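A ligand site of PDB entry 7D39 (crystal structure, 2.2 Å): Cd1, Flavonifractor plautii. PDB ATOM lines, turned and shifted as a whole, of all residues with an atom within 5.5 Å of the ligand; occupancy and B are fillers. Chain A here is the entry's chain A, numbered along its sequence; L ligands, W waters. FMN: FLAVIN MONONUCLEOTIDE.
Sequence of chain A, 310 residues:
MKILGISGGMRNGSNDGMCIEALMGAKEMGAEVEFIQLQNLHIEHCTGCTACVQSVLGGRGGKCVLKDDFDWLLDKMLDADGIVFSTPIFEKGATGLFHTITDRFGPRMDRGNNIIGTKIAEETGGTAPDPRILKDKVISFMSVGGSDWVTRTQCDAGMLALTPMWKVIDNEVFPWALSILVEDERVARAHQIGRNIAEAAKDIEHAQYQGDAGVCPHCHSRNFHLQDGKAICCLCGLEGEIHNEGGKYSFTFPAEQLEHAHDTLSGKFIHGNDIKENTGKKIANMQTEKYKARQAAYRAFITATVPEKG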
ATOM      1  N   SER A   7     -22.239   0.316  13.196  1.00  0.00           N
ATOM      2  CA  SER A   7     -22.991  -0.269  12.098  1.00  0.00           C
ATOM      3  C   SER A   7     -24.216   0.584  11.797  1.00  0.00           C
ATOM      4  O   SER A   7     -24.973   0.930  12.709  1.00  0.00           O
ATOM      5  CB  SER A   7     -23.403  -1.701  12.401  1.00  0.00           C
ATOM      6  OG  SER A   7     -24.427  -2.091  11.521  1.00  0.00           O
ATOM      7  N   GLY A   9     -26.582  -0.557   9.553  1.00  0.00           N
ATOM      8  CA  GLY A   9     -27.597  -1.438   9.010  1.00  0.00           C
ATOM      9  C   GLY A   9     -28.722  -1.682  10.002  1.00  0.00           C
ATOM     10  O   GLY A   9     -28.821  -1.040  11.048  1.00  0.00           O
ATOM     11  N   MET A  10     -29.595  -2.636   9.650  1.00  0.00           N
ATOM     12  CA  MET A  10     -30.640  -3.037  10.585  1.00  0.00           C
ATOM     13  C   MET A  10     -30.051  -3.798  11.776  1.00  0.00           C
ATOM     14  O   MET A  10     -29.003  -4.447  11.655  1.00  0.00           O
ATOM     15  CB  MET A  10     -31.693  -3.921   9.896  1.00  0.00           C
ATOM     16  CG  MET A  10     -32.677  -3.212   8.951  1.00  0.00           C
ATOM     17  SD  MET A  10     -33.725  -1.750   9.726  1.00  0.00           S
ATOM     18  CE  MET A  10     -33.930  -2.398  11.571  1.00  0.00           C
ATOM     19  N   GLY A  13     -28.376  -7.367  11.450  1.00  0.00           N
ATOM     20  CA  GLY A  13     -28.222  -7.602  10.026  1.00  0.00           C
ATOM     21  C   GLY A  13     -26.783  -7.858   9.649  1.00  0.00           C
ATOM     22  O   GLY A  13     -25.912  -8.103  10.484  1.00  0.00           O
ATOM     23  N   SER A  14     -26.527  -7.773   8.335  1.00  0.00           N
ATOM     24  CA  SER A  14     -25.209  -8.111   7.808  1.00  0.00           C
ATOM     25  C   SER A  14     -24.159  -7.065   8.189  1.00  0.00           C
ATOM     26  O   SER A  14     -23.003  -7.415   8.483  1.00  0.00           O
ATOM     27  CB  SER A  14     -25.306  -8.280   6.298  1.00  0.00           C
ATOM     28  OG  SER A  14     -26.167  -9.382   5.989  1.00  0.00           O
ATOM     29  N   ASN A  15     -24.510  -5.785   8.187  1.00  0.00           N
ATOM     30  CA  ASN A  15     -23.528  -4.776   8.600  1.00  0.00           C
ATOM     31  C   ASN A  15     -23.115  -4.967  10.054  1.00  0.00           C
ATOM     32  O   ASN A  15     -21.940  -4.800  10.399  1.00  0.00           O
ATOM     33  CB  ASN A  15     -24.068  -3.366   8.346  1.00  0.00           C
ATOM     34  CG  ASN A  15     -24.016  -2.992   6.868  1.00  0.00           C
ATOM     35  OD1 ASN A  15     -23.013  -2.447   6.391  1.00  0.00           O
ATOM     36  ND2 ASN A  15     -25.091  -3.307   6.130  1.00  0.00           N
ATOM     37  N   ASP A  16     -24.073  -5.283  10.940  1.00  0.00           N
ATOM     38  CA  ASP A  16     -23.731  -5.591  12.322  1.00  0.00           C
ATOM     39  C   ASP A  16     -22.725  -6.724  12.382  1.00  0.00           C
ATOM     40  O   ASP A  16     -21.702  -6.634  13.067  1.00  0.00           O
ATOM     41  CB  ASP A  16     -24.985  -5.992  13.121  1.00  0.00           C
ATOM     42  CG  ASP A  16     -25.840  -4.795  13.552  1.00  0.00           C
ATOM     43  OD1 ASP A  16     -25.647  -3.656  13.080  1.00  0.00           O
ATOM     44  OD2 ASP A  16     -26.753  -5.017  14.373  1.00  0.00           O
ATOM     45  N   PRO A  88     -24.691   0.142   5.148  1.00  0.00           N
ATOM     46  CA  PRO A  88     -25.412  -0.311   3.953  1.00  0.00           C
ATOM     47  C   PRO A  88     -25.147   0.630   2.782  1.00  0.00           C
ATOM     48  O   PRO A  88     -24.774   1.787   2.964  1.00  0.00           O
ATOM     49  CB  PRO A  88     -26.891  -0.242   4.372  1.00  0.00           C
ATOM     50  CG  PRO A  88     -26.889  -0.035   5.840  1.00  0.00           C
ATOM     51  CD  PRO A  88     -25.586   0.517   6.246  1.00  0.00           C
ATOM     52  N   ILE A  89     -25.366   0.120   1.581  1.00  0.00           N
ATOM     53  CA  ILE A  89     -25.343   0.920   0.361  1.00  0.00           C
ATOM     54  C   ILE A  89     -26.792   1.216  -0.013  1.00  0.00           C
ATOM     55  O   ILE A  89     -27.608   0.300  -0.152  1.00  0.00           O
ATOM     56  CB  ILE A  89     -24.612   0.192  -0.765  1.00  0.00           C
ATOM     57  CG1 ILE A  89     -23.178  -0.120  -0.348  1.00  0.00           C
ATOM     58  CG2 ILE A  89     -24.666   1.028  -2.049  1.00  0.00           C
ATOM     59  CD1 ILE A  89     -22.384  -0.888  -1.367  1.00  0.00           C
ATOM     60  N   PHE A  90     -27.121   2.503  -0.161  1.00  0.00           N
ATOM     61  CA  PHE A  90     -28.427   2.968  -0.639  1.00  0.00           C
ATOM     62  C   PHE A  90     -28.177   3.791  -1.908  1.00  0.00           C
ATOM     63  O   PHE A  90     -27.384   4.737  -1.880  1.00  0.00           O
ATOM     64  CB  PHE A  90     -29.135   3.868   0.399  1.00  0.00           C
ATOM     65  CG  PHE A  90     -29.701   3.144   1.607  1.00  0.00           C
ATOM     66  CD1 PHE A  90     -29.615   1.763   1.774  1.00  0.00           C
ATOM     67  CD2 PHE A  90     -30.337   3.889   2.609  1.00  0.00           C
ATOM     68  CE1 PHE A  90     -30.157   1.143   2.909  1.00  0.00           C
ATOM     69  CE2 PHE A  90     -30.870   3.279   3.743  1.00  0.00           C
ATOM     70  CZ  PHE A  90     -30.774   1.896   3.898  1.00  0.00           C
ATOM     71  N   GLU A  91     -28.825   3.425  -3.019  1.00  0.00           N
ATOM     72  CA  GLU A  91     -28.660   4.127  -4.297  1.00  0.00           C
ATOM     73  C   GLU A  91     -27.193   4.387  -4.634  1.00  0.00           C
ATOM     74  O   GLU A  91     -26.794   5.505  -4.978  1.00  0.00           O
ATOM     75  CB  GLU A  91     -29.457   5.432  -4.318  1.00  0.00           C
ATOM     76  CG  GLU A  91     -30.952   5.206  -4.052  1.00  0.00           C
ATOM     77  CD  GLU A  91     -31.295   5.386  -2.599  1.00  0.00           C
ATOM     78  OE1 GLU A  91     -30.774   6.349  -1.993  1.00  0.00           O
ATOM     79  OE2 GLU A  91     -32.083   4.594  -2.045  1.00  0.00           O
ATOM     80  N   LYS A  92     -26.368   3.343  -4.509  1.00  0.00           N
ATOM     81  CA  LYS A  92     -24.968   3.384  -4.939  1.00  0.00           C
ATOM     82  C   LYS A  92     -24.198   4.414  -4.117  1.00  0.00           C
ATOM     83  O   LYS A  92     -23.448   5.227  -4.668  1.00  0.00           O
ATOM     84  CB  LYS A  92     -24.826   4.144  -6.250  1.00  0.00           C
ATOM     85  CG  LYS A  92     -25.371   3.369  -7.427  1.00  0.00           C
ATOM     86  CD  LYS A  92     -25.475   4.272  -8.630  1.00  0.00           C
ATOM     87  CE  LYS A  92     -26.193   3.565  -9.752  1.00  0.00           C
ATOM     88  NZ  LYS A  92     -26.520   4.458 -10.886  1.00  0.00           N
ATOM     89  N   GLY A  93     -24.390   4.399  -2.796  1.00  0.00           N
ATOM     90  CA  GLY A  93     -23.684   5.369  -1.991  1.00  0.00           C
ATOM     91  C   GLY A  93     -24.018   4.912  -0.583  1.00  0.00           C
ATOM     92  O   GLY A  93     -24.657   3.873  -0.398  1.00  0.00           O
ATOM     93  N   VAL A 144     -21.652  -2.337   2.388  1.00  0.00           N
ATOM     94  CA  VAL A 144     -22.262  -3.640   2.107  1.00  0.00           C
ATOM     95  C   VAL A 144     -23.566  -3.400   1.366  1.00  0.00           C
ATOM     96  O   VAL A 144     -24.474  -2.757   1.885  1.00  0.00           O
ATOM     97  CB  VAL A 144     -22.519  -4.441   3.396  1.00  0.00           C
ATOM     98  CG1 VAL A 144     -23.029  -5.832   3.050  1.00  0.00           C
ATOM     99  CG2 VAL A 144     -21.247  -4.498   4.256  1.00  0.00           C
ATOM    100  N   GLY A 145     -23.657  -3.945   0.142  1.00  0.00           N
ATOM    101  CA  GLY A 145     -24.812  -3.736  -0.695  1.00  0.00           C
ATOM    102  C   GLY A 145     -25.476  -5.048  -1.080  1.00  0.00           C
ATOM    103  O   GLY A 145     -24.911  -6.128  -0.939  1.00  0.00           O
ATOM    104  N   GLY A 146     -26.703  -4.928  -1.586  1.00  0.00           N
ATOM    105  CA  GLY A 146     -27.392  -6.094  -2.123  1.00  0.00           C
ATOM    106  C   GLY A 146     -27.009  -6.462  -3.543  1.00  0.00           C
ATOM    107  O   GLY A 146     -27.136  -7.622  -3.937  1.00  0.00           O
ATOM    108  N   SER A 147     -26.526  -5.497  -4.328  1.00  0.00           N
ATOM    109  CA  SER A 147     -26.272  -5.714  -5.757  1.00  0.00           C
ATOM    110  C   SER A 147     -24.888  -5.219  -6.165  1.00  0.00           C
ATOM    111  O   SER A 147     -23.981  -5.174  -5.341  1.00  0.00           O
ATOM    112  CB  SER A 147     -27.325  -5.026  -6.610  1.00  0.00           C
ATOM    113  OG  SER A 147     -27.146  -3.610  -6.590  1.00  0.00           O
ATOM    114  N   ASP A 148     -24.712  -4.868  -7.443  1.00  0.00           N
ATOM    115  CA  ASP A 148     -23.491  -4.224  -7.896  1.00  0.00           C
ATOM    116  C   ASP A 148     -23.673  -2.716  -8.123  1.00  0.00           C
ATOM    117  O   ASP A 148     -22.815  -2.082  -8.742  1.00  0.00           O
ATOM    118  CB  ASP A 148     -22.967  -4.901  -9.164  1.00  0.00           C
ATOM    119  CG  ASP A 148     -23.903  -4.758 -10.346  1.00  0.00           C
ATOM    120  OD1 ASP A 148     -25.028  -4.264 -10.171  1.00  0.00           O
ATOM    121  OD2 ASP A 148     -23.525  -5.179 -11.467  1.00  0.00           O
ATOM    122  N   TRP A 149     -24.757  -2.142  -7.626  1.00  0.00           N
ATOM    123  CA  TRP A 149     -24.968  -0.697  -7.672  1.00  0.00           C
ATOM    124  C   TRP A 149     -24.216  -0.096  -6.494  1.00  0.00           C
ATOM    125  O   TRP A 149     -24.786   0.171  -5.437  1.00  0.00           O
ATOM    126  CB  TRP A 149     -26.452  -0.359  -7.600  1.00  0.00           C
ATOM    127  CG  TRP A 149     -27.299  -0.747  -8.765  1.00  0.00           C
ATOM    128  CD1 TRP A 149     -27.081  -1.769  -9.670  1.00  0.00           C
ATOM    129  CD2 TRP A 149     -28.503  -0.108  -9.191  1.00  0.00           C
ATOM    130  NE1 TRP A 149     -28.082  -1.792 -10.606  1.00  0.00           N
ATOM    131  CE2 TRP A 149     -28.962  -0.781 -10.337  1.00  0.00           C
ATOM    132  CE3 TRP A 149     -29.235   0.991  -8.715  1.00  0.00           C
ATOM    133  CZ2 TRP A 149     -30.132  -0.405 -11.006  1.00  0.00           C
ATOM    134  CZ3 TRP A 149     -30.394   1.357  -9.374  1.00  0.00           C
ATOM    135  CH2 TRP A 149     -30.831   0.665 -10.511  1.00  0.00           C
ATOM    136  N   VAL A 150     -22.914   0.120  -6.685  1.00  0.00           N
ATOM    137  CA  VAL A 150     -22.024   0.394  -5.556  1.00  0.00           C
ATOM    138  C   VAL A 150     -20.939   1.434  -5.876  1.00  0.00           C
ATOM    139  O   VAL A 150     -19.891   1.461  -5.219  1.00  0.00           O
ATOM    140  CB  VAL A 150     -21.384  -0.917  -5.080  1.00  0.00           C
ATOM    141  CG1 VAL A 150     -22.481  -1.967  -4.767  1.00  0.00           C
ATOM    142  CG2 VAL A 150     -20.459  -1.450  -6.147  1.00  0.00           C
ATOM    143  N   TRP A 176     -23.292  -7.581  -3.900  1.00  0.00           N
ATOM    144  CA  TRP A 176     -24.027  -8.855  -3.885  1.00  0.00           C
ATOM    145  C   TRP A 176     -23.928  -9.523  -2.521  1.00  0.00           C
ATOM    146  O   TRP A 176     -23.653 -10.722  -2.415  1.00  0.00           O
ATOM    147  CB  TRP A 176     -23.518  -9.807  -4.974  1.00  0.00           C
ATOM    148  CG  TRP A 176     -23.569  -9.231  -6.346  1.00  0.00           C
ATOM    149  CD1 TRP A 176     -22.506  -8.856  -7.129  1.00  0.00           C
ATOM    150  CD2 TRP A 176     -24.744  -8.955  -7.116  1.00  0.00           C
ATOM    151  NE1 TRP A 176     -22.952  -8.360  -8.333  1.00  0.00           N
ATOM    152  CE2 TRP A 176     -24.326  -8.403  -8.351  1.00  0.00           C
ATOM    153  CE3 TRP A 176     -26.120  -9.125  -6.880  1.00  0.00           C
ATOM    154  CZ2 TRP A 176     -25.213  -8.022  -9.349  1.00  0.00           C
ATOM    155  CZ3 TRP A 176     -27.006  -8.733  -7.868  1.00  0.00           C
ATOM    156  CH2 TRP A 176     -26.546  -8.190  -9.088  1.00  0.00           C
ATOM    157  N   LEU A 178     -26.174  -9.685   0.260  1.00  0.00           N
ATOM    158  CA  LEU A 178     -27.310 -10.013   1.099  1.00  0.00           C
ATOM    159  C   LEU A 178     -27.051 -11.267   1.910  1.00  0.00           C
ATOM    160  O   LEU A 178     -27.478 -11.374   3.065  1.00  0.00           O
ATOM    161  CB  LEU A 178     -28.584 -10.183   0.270  1.00  0.00           C
ATOM    162  CG  LEU A 178     -29.344  -8.977  -0.262  1.00  0.00           C
ATOM    163  CD1 LEU A 178     -30.714  -9.446  -0.748  1.00  0.00           C
ATOM    164  CD2 LEU A 178     -29.503  -7.913   0.783  1.00  0.00           C
HETATM  165  N1  FMN L   1     -27.816  -2.345  -2.484  1.00  0.00           N
HETATM  166  C2  FMN L   1     -26.930  -2.126  -3.454  1.00  0.00           C
HETATM  167  O2  FMN L   1     -26.139  -3.059  -3.547  1.00  0.00           O
HETATM  168  N3  FMN L   1     -26.955  -1.002  -4.221  1.00  0.00           N
HETATM  169  C4  FMN L   1     -27.899  -0.061  -3.968  1.00  0.00           C
HETATM  170  O4  FMN L   1     -28.046   0.989  -4.572  1.00  0.00           O
HETATM  171  C4A FMN L   1     -28.884  -0.290  -2.905  1.00  0.00           C
HETATM  172  N5  FMN L   1     -29.834   0.564  -2.612  1.00  0.00           N
HETATM  173  C5A FMN L   1     -30.707   0.396  -1.629  1.00  0.00           C
HETATM  174  C6  FMN L   1     -31.695   1.321  -1.328  1.00  0.00           C
HETATM  175  C7  FMN L   1     -32.603   1.118  -0.297  1.00  0.00           C
HETATM  176  C7M FMN L   1     -33.671   2.124  -0.004  1.00  0.00           C
HETATM  177  C8  FMN L   1     -32.530  -0.146   0.478  1.00  0.00           C
HETATM  178  C8M FMN L   1     -33.521  -0.392   1.584  1.00  0.00           C
HETATM  179  C9  FMN L   1     -31.553  -1.073   0.168  1.00  0.00           C
HETATM  180  C9A FMN L   1     -30.643  -0.848  -0.845  1.00  0.00           C
HETATM  181  N10 FMN L   1     -29.667  -1.795  -1.163  1.00  0.00           N
HETATM  182  C10 FMN L   1     -28.774  -1.509  -2.169  1.00  0.00           C
HETATM  183  C1' FMN L   1     -29.589  -3.006  -0.353  1.00  0.00           C
HETATM  184  C2' FMN L   1     -28.866  -2.731   0.979  1.00  0.00           C
HETATM  185  O2' FMN L   1     -27.517  -2.344   0.807  1.00  0.00           O
HETATM  186  C3' FMN L   1     -29.002  -3.946   1.937  1.00  0.00           C
HETATM  187  O3' FMN L   1     -30.337  -4.187   2.276  1.00  0.00           O
HETATM  188  C4' FMN L   1     -28.119  -3.810   3.201  1.00  0.00           C
HETATM  189  O4' FMN L   1     -26.738  -4.016   2.918  1.00  0.00           O
HETATM  190  C5' FMN L   1     -28.605  -4.757   4.289  1.00  0.00           C
HETATM  191  O5' FMN L   1     -27.829  -4.690   5.441  1.00  0.00           O
HETATM  192  P   FMN L   1     -28.186  -4.993   6.879  1.00  0.00           P
HETATM  193  O1P FMN L   1     -27.112  -4.631   7.684  1.00  0.00           O
HETATM  194  O2P FMN L   1     -29.308  -4.206   7.189  1.00  0.00           O
HETATM  195  O3P FMN L   1     -28.336  -6.410   6.845  1.00  0.00           O
HETATM  196  O   HOH W   1     -28.139  -8.270   4.704  1.00  0.00           O
HETATM  197  O   HOH W   2     -31.831  -5.498   6.425  1.00  0.00           O
HETATM  198  O   HOH W   3     -29.889  -1.773   5.723  1.00  0.00           O
HETATM  199  O   HOH W   4     -26.705  -4.566  10.279  1.00  0.00           O
HETATM  200  O   HOH W   5     -31.732  -6.544   3.301  1.00  0.00           O
HETATM  201  O   HOH W   6     -31.434  -2.406   3.665  1.00  0.00           O
HETATM  202  O   HOH W   7     -26.635  -7.119   2.825  1.00  0.00           O
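Residues that only touch the ligand: Gly 9 (3.5 Å), Gly 13 (3.4 Å), Pro 88 (3.95 Å), Phe 90 (3.4 Å) and Gly 145 (3.2 Å). Hydrophobic or aromatic side chains within 4 Å of the ligand: Met 10, Pro 88, Ile 89, Phe 90 and Trp 149. Of the 22 residues printed, 15 come within 4 Å of the ligand.
The backbone NH (N) of Trp 149 is in hydrogen-bond range of the side-chain hydroxyl (OG) of Ser 147 (3.0 Å). O of Ser 147 sits at hydrogen-bond distance from N of Trp 176, at 2.9 Å. O of Val 144 is in hydrogen-bond range of N of Ile 89 (3.0 Å). N of Gly 9 sits at hydrogen-bond distance from OG of Ser 7, 3.3 Å away.
O2 of the ligand lies within hydrogen-bond range of N of Ser 147, 2.6 Å away. An oxygen (O2) of the ligand lies within hydrogen-bond range of the side-chain hydroxyl (OG) of Ser 147, at 3.3 Å. An oxygen (O3P) of the ligand lies within hydrogen-bond range of the backbone NH of Ser 14, 2.7 Å away. A nitrogen (N3) of the ligand lies within hydrogen-bond range of the backbone carbonyl oxygen (O) of Trp 149, at 2.7 Å. An oxygen (O2) of the ligand is in hydrogen-bond range of the backbone NH (N) of Gly 146 (2.8 Å). The backbone carbonyl oxygen (O) of Val 144 is in hydrogen-bond range of an oxygen (O4') of the ligand (2.8 Å). The backbone NH (N) of Ile 89 lies within hydrogen-bond range of an oxygen (O2') of the ligand (3.4 Å). The backbone carbonyl oxygen (O) of Ile 89 sits at hydrogen-bond distance from an oxygen (O2') of the ligand. An oxygen (O1P) of the ligand lies within hydrogen-bond range of the backbone NH (N) of Asn 15 (2.9 Å). ND2 of Asn 15 is in hydrogen-bond range of O1P of the ligand (2.9 Å). The backbone NH (N) of Lys 92 is in hydrogen-bond range of an oxygen (O4) of the ligand (2.9 Å). The backbone NH (N) of Met 10 is in hydrogen-bond range of an oxygen (O2P) of the ligand, 2.9 Å away. The backbone NH (N) of Glu 91 lies within hydrogen-bond range of an oxygen (O4) of the ligand (3.0 Å).
Water W1 lies within hydrogen-bond range of OG of Ser 14 (2.6 Å) and O3P of the ligand (2.8 Å).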
